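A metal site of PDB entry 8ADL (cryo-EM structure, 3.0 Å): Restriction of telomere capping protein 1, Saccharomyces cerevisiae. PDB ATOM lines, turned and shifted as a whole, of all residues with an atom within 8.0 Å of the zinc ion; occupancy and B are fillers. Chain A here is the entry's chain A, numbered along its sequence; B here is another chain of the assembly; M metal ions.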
ATOM      1  N   SER A1292      25.728 -26.859   2.080  1.00  0.00           N
ATOM      2  CA  SER A1292      26.059 -28.121   1.445  1.00  0.00           C
ATOM      3  C   SER A1292      25.755 -28.071  -0.052  1.00  0.00           C
ATOM      4  O   SER A1292      24.818 -27.405  -0.488  1.00  0.00           O
ATOM      5  CB  SER A1292      25.284 -29.267   2.088  1.00  0.00           C
ATOM      6  OG  SER A1292      25.656 -29.435   3.446  1.00  0.00           O
ATOM      7  N   CYS A1293      26.588 -28.764  -0.822  1.00  0.00           N
ATOM      8  CA  CYS A1293      26.357 -28.884  -2.260  1.00  0.00           C
ATOM      9  C   CYS A1293      25.103 -29.697  -2.528  1.00  0.00           C
ATOM     10  O   CYS A1293      24.760 -30.611  -1.763  1.00  0.00           O
ATOM     11  CB  CYS A1293      27.567 -29.524  -2.937  1.00  0.00           C
ATOM     12  SG  CYS A1293      27.446 -29.662  -4.739  1.00  0.00           S
ATOM     13  N   VAL A1294      24.416 -29.359  -3.609  1.00  0.00           N
ATOM     14  CA  VAL A1294      23.163 -30.037  -3.935  1.00  0.00           C
ATOM     15  C   VAL A1294      23.400 -31.428  -4.527  1.00  0.00           C
ATOM     16  O   VAL A1294      22.489 -32.258  -4.534  1.00  0.00           O
ATOM     17  CB  VAL A1294      22.339 -29.145  -4.878  1.00  0.00           C
ATOM     18  CG1 VAL A1294      22.888 -29.171  -6.296  1.00  0.00           C
ATOM     19  CG2 VAL A1294      20.859 -29.502  -4.838  1.00  0.00           C
ATOM     20  N   LEU A1295      24.625 -31.725  -4.973  1.00  0.00           N
ATOM     21  CA  LEU A1295      24.948 -33.017  -5.551  1.00  0.00           C
ATOM     22  C   LEU A1295      25.782 -33.903  -4.621  1.00  0.00           C
ATOM     23  O   LEU A1295      25.398 -35.044  -4.362  1.00  0.00           O
ATOM     24  CB  LEU A1295      25.701 -32.832  -6.877  1.00  0.00           C
ATOM     25  CG  LEU A1295      25.733 -34.057  -7.792  1.00  0.00           C
ATOM     26  CD1 LEU A1295      24.342 -34.430  -8.256  1.00  0.00           C
ATOM     27  CD2 LEU A1295      26.650 -33.831  -8.977  1.00  0.00           C
ATOM     28  N   CYS A1296      26.899 -33.395  -4.107  1.00  0.00           N
ATOM     29  CA  CYS A1296      27.824 -34.198  -3.316  1.00  0.00           C
ATOM     30  C   CYS A1296      27.651 -34.028  -1.815  1.00  0.00           C
ATOM     31  O   CYS A1296      28.258 -34.803  -1.055  1.00  0.00           O
ATOM     32  CB  CYS A1296      29.270 -33.869  -3.704  1.00  0.00           C
ATOM     33  SG  CYS A1296      29.804 -32.198  -3.299  1.00  0.00           S
ATOM     34  N   GLU A1297      26.859 -33.044  -1.365  1.00  0.00           N
ATOM     35  CA  GLU A1297      26.554 -32.800   0.046  1.00  0.00           C
ATOM     36  C   GLU A1297      27.808 -32.536   0.884  1.00  0.00           C
ATOM     37  O   GLU A1297      27.869 -32.909   2.054  1.00  0.00           O
ATOM     38  CB  GLU A1297      25.726 -33.930   0.655  1.00  0.00           C
ATOM     39  CG  GLU A1297      24.319 -34.045   0.101  1.00  0.00           C
ATOM     40  CD  GLU A1297      23.414 -32.915   0.552  1.00  0.00           C
ATOM     41  OE1 GLU A1297      23.579 -32.445   1.702  1.00  0.00           O
ATOM     42  OE2 GLU A1297      22.547 -32.504  -0.231  1.00  0.00           O
ATOM     43  N   ARG A1298      28.812 -31.915   0.278  1.00  0.00           N
ATOM     44  CA  ARG A1298      30.055 -31.518   0.907  1.00  0.00           C
ATOM     45  C   ARG A1298      30.021 -30.040   1.259  1.00  0.00           C
ATOM     46  O   ARG A1298      29.183 -29.295   0.736  1.00  0.00           O
ATOM     47  CB  ARG A1298      31.231 -31.820  -0.031  1.00  0.00           C
ATOM     48  CG  ARG A1298      31.766 -33.234   0.065  1.00  0.00           C
ATOM     49  CD  ARG A1298      32.835 -33.490  -0.973  1.00  0.00           C
ATOM     50  NE  ARG A1298      32.809 -34.856  -1.483  1.00  0.00           N
ATOM     51  CZ  ARG A1298      33.284 -35.230  -2.651  1.00  0.00           C
ATOM     52  NH1 ARG A1298      33.836 -34.359  -3.487  1.00  0.00           N
ATOM     53  NH2 ARG A1298      33.206 -36.510  -3.009  1.00  0.00           N
ATOM     54  N   PRO A1299      30.875 -29.572   2.170  1.00  0.00           N
ATOM     55  CA  PRO A1299      30.910 -28.135   2.485  1.00  0.00           C
ATOM     56  C   PRO A1299      31.331 -27.295   1.286  1.00  0.00           C
ATOM     57  O   PRO A1299      32.106 -27.731   0.433  1.00  0.00           O
ATOM     58  CB  PRO A1299      31.942 -28.036   3.626  1.00  0.00           C
ATOM     59  CG  PRO A1299      32.663 -29.339   3.616  1.00  0.00           C
ATOM     60  CD  PRO A1299      31.671 -30.339   3.153  1.00  0.00           C
ATOM     61  N   LEU A1300      30.812 -26.073   1.242  1.00  0.00           N
ATOM     62  CA  LEU A1300      30.947 -25.200   0.088  1.00  0.00           C
ATOM     63  C   LEU A1300      31.315 -23.812   0.578  1.00  0.00           C
ATOM     64  O   LEU A1300      30.534 -23.180   1.295  1.00  0.00           O
ATOM     65  CB  LEU A1300      29.640 -25.168  -0.716  1.00  0.00           C
ATOM     66  CG  LEU A1300      29.665 -24.582  -2.122  1.00  0.00           C
ATOM     67  CD1 LEU A1300      30.874 -25.070  -2.890  1.00  0.00           C
ATOM     68  CD2 LEU A1300      28.390 -24.968  -2.849  1.00  0.00           C
ATOM     69  N   LEU A1303      33.450 -21.028  -4.077  1.00  0.00           N
ATOM     70  CA  LEU A1303      32.781 -20.723  -5.341  1.00  0.00           C
ATOM     71  C   LEU A1303      31.589 -21.654  -5.493  1.00  0.00           C
ATOM     72  O   LEU A1303      31.723 -22.873  -5.332  1.00  0.00           O
ATOM     73  CB  LEU A1303      33.724 -20.877  -6.544  1.00  0.00           C
ATOM     74  CG  LEU A1303      34.401 -19.625  -7.102  1.00  0.00           C
ATOM     75  CD1 LEU A1303      35.465 -20.002  -8.124  1.00  0.00           C
ATOM     76  CD2 LEU A1303      33.389 -18.673  -7.714  1.00  0.00           C
ATOM     77  N   GLU A1313      22.715 -24.257  -4.306  1.00  0.00           N
ATOM     78  CA  GLU A1313      24.129 -24.014  -4.566  1.00  0.00           C
ATOM     79  C   GLU A1313      24.719 -25.186  -5.347  1.00  0.00           C
ATOM     80  O   GLU A1313      24.007 -26.063  -5.853  1.00  0.00           O
ATOM     81  CB  GLU A1313      24.891 -23.786  -3.273  1.00  0.00           C
ATOM     82  CG  GLU A1313      24.218 -22.918  -2.235  1.00  0.00           C
ATOM     83  CD  GLU A1313      24.534 -21.456  -2.380  1.00  0.00           C
ATOM     84  OE1 GLU A1313      25.350 -21.097  -3.247  1.00  0.00           O
ATOM     85  OE2 GLU A1313      24.008 -20.656  -1.583  1.00  0.00           O
ATOM     86  N   GLY A1314      26.042 -25.219  -5.445  1.00  0.00           N
ATOM     87  CA  GLY A1314      26.750 -26.337  -6.059  1.00  0.00           C
ATOM     88  C   GLY A1314      28.111 -25.938  -6.574  1.00  0.00           C
ATOM     89  O   GLY A1314      28.310 -24.793  -6.976  1.00  0.00           O
ATOM     90  N   HIS A1315      29.059 -26.874  -6.587  1.00  0.00           N
ATOM     91  CA  HIS A1315      30.368 -26.620  -7.168  1.00  0.00           C
ATOM     92  C   HIS A1315      30.262 -26.458  -8.683  1.00  0.00           C
ATOM     93  O   HIS A1315      29.241 -26.794  -9.295  1.00  0.00           O
ATOM     94  CB  HIS A1315      31.338 -27.756  -6.853  1.00  0.00           C
ATOM     95  CG  HIS A1315      31.516 -28.023  -5.389  1.00  0.00           C
ATOM     96  ND1 HIS A1315      30.605 -28.733  -4.644  1.00  0.00           N
ATOM     97  CD2 HIS A1315      32.523 -27.709  -4.546  1.00  0.00           C
ATOM     98  CE1 HIS A1315      31.029 -28.826  -3.397  1.00  0.00           C
ATOM     99  NE2 HIS A1315      32.194 -28.209  -3.303  1.00  0.00           N
ATOM    100  N   PHE A1316      31.332 -25.921  -9.279  1.00  0.00           N
ATOM    101  CA  PHE A1316      31.425 -25.924 -10.735  1.00  0.00           C
ATOM    102  C   PHE A1316      31.445 -27.337 -11.287  1.00  0.00           C
ATOM    103  O   PHE A1316      30.720 -27.663 -12.238  1.00  0.00           O
ATOM    104  CB  PHE A1316      32.658 -25.152 -11.204  1.00  0.00           C
ATOM    105  CG  PHE A1316      32.595 -23.670 -10.991  1.00  0.00           C
ATOM    106  CD1 PHE A1316      31.391 -23.033 -10.713  1.00  0.00           C
ATOM    107  CD2 PHE A1316      33.738 -22.893 -11.087  1.00  0.00           C
ATOM    108  CE1 PHE A1316      31.337 -21.673 -10.537  1.00  0.00           C
ATOM    109  CE2 PHE A1316      33.687 -21.522 -10.903  1.00  0.00           C
ATOM    110  CZ  PHE A1316      32.486 -20.916 -10.622  1.00  0.00           C
ATOM    111  N   GLN A1317      32.256 -28.209 -10.682  1.00  0.00           N
ATOM    112  CA  GLN A1317      32.419 -29.562 -11.195  1.00  0.00           C
ATOM    113  C   GLN A1317      31.143 -30.375 -11.040  1.00  0.00           C
ATOM    114  O   GLN A1317      30.748 -31.093 -11.966  1.00  0.00           O
ATOM    115  CB  GLN A1317      33.594 -30.255 -10.500  1.00  0.00           C
ATOM    116  CG  GLN A1317      34.062 -31.521 -11.187  1.00  0.00           C
ATOM    117  CD  GLN A1317      34.651 -31.259 -12.556  1.00  0.00           C
ATOM    118  OE1 GLN A1317      35.357 -30.278 -12.768  1.00  0.00           O
ATOM    119  NE2 GLN A1317      34.359 -32.147 -13.510  1.00  0.00           N
ATOM    120  N   CYS A1318      30.463 -30.253  -9.898  1.00  0.00           N
ATOM    121  CA  CYS A1318      29.250 -31.031  -9.636  1.00  0.00           C
ATOM    122  C   CYS A1318      28.114 -30.621 -10.567  1.00  0.00           C
ATOM    123  O   CYS A1318      27.480 -31.474 -11.212  1.00  0.00           O
ATOM    124  CB  CYS A1318      28.833 -30.860  -8.176  1.00  0.00           C
ATOM    125  SG  CYS A1318      30.054 -31.431  -6.983  1.00  0.00           S
ATOM    126  N   ILE A1319      27.845 -29.311 -10.655  1.00  0.00           N
ATOM    127  CA  ILE A1319      26.775 -28.797 -11.499  1.00  0.00           C
ATOM    128  C   ILE A1319      27.076 -29.062 -12.978  1.00  0.00           C
ATOM    129  O   ILE A1319      26.196 -29.461 -13.739  1.00  0.00           O
ATOM    130  CB  ILE A1319      26.551 -27.302 -11.208  1.00  0.00           C
ATOM    131  CG1 ILE A1319      25.975 -27.108  -9.806  1.00  0.00           C
ATOM    132  CG2 ILE A1319      25.637 -26.663 -12.237  1.00  0.00           C
ATOM    133  CD1 ILE A1319      24.635 -27.767  -9.609  1.00  0.00           C
ATOM    134  N   GLU A1321      28.998 -31.482 -14.217  1.00  0.00           N
ATOM    135  CA  GLU A1321      28.850 -32.916 -14.462  1.00  0.00           C
ATOM    136  C   GLU A1321      27.383 -33.292 -14.585  1.00  0.00           C
ATOM    137  O   GLU A1321      26.988 -34.002 -15.523  1.00  0.00           O
ATOM    138  CB  GLU A1321      29.516 -33.706 -13.332  1.00  0.00           C
ATOM    139  CG  GLU A1321      30.993 -33.995 -13.546  1.00  0.00           C
ATOM    140  CD  GLU A1321      31.625 -34.664 -12.343  1.00  0.00           C
ATOM    141  OE1 GLU A1321      30.961 -34.735 -11.292  1.00  0.00           O
ATOM    142  OE2 GLU A1321      32.778 -35.129 -12.450  1.00  0.00           O
ATOM    143  N   PHE B 847      26.627 -39.963  -6.408  1.00  0.00           N
ATOM    144  CA  PHE B 847      25.844 -38.748  -6.182  1.00  0.00           C
ATOM    145  C   PHE B 847      24.840 -38.498  -7.310  1.00  0.00           C
ATOM    146  O   PHE B 847      23.747 -37.992  -7.065  1.00  0.00           O
ATOM    147  CB  PHE B 847      26.784 -37.558  -6.020  1.00  0.00           C
ATOM    148  CG  PHE B 847      27.805 -37.747  -4.943  1.00  0.00           C
ATOM    149  CD1 PHE B 847      27.431 -37.937  -3.629  1.00  0.00           C
ATOM    150  CD2 PHE B 847      29.163 -37.727  -5.247  1.00  0.00           C
ATOM    151  CE1 PHE B 847      28.371 -38.112  -2.633  1.00  0.00           C
ATOM    152  CE2 PHE B 847      30.111 -37.905  -4.261  1.00  0.00           C
ATOM    153  CZ  PHE B 847      29.714 -38.102  -2.953  1.00  0.00           C
HETATM  154 ZN    ZN M   1      29.586 -30.541  -4.900  1.00  0.00          ZN
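Within 4 Å of the zinc ion: Cys 1293, Cys 1296, His 1315 and Cys 1318.
The backbone NH (N) of Cys 1293 is in hydrogen-bond range of the backbone carbonyl oxygen (O) of Arg 1298, at 3.1 Å.
The side-chain sulfur (SG) of Cys 1296 sits close to the backbone NH (N) of Arg 1298 (3.7 Å).
The side-chain sulfur (SG) of Cys 1293 lies close to the backbone NH (N) of Leu 1295, 3.5 Å away.
The zinc ion is bound by a ring nitrogen (ND1) of His 1315 (2.1 Å), the side-chain sulfur of Cys 1318 (2.3 Å), the side-chain sulfur of Cys 1296 (2.3 Å) and the side-chain sulfur of Cys 1293 (2.3 Å).
The zinc ion has four donor atoms within binding distance.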
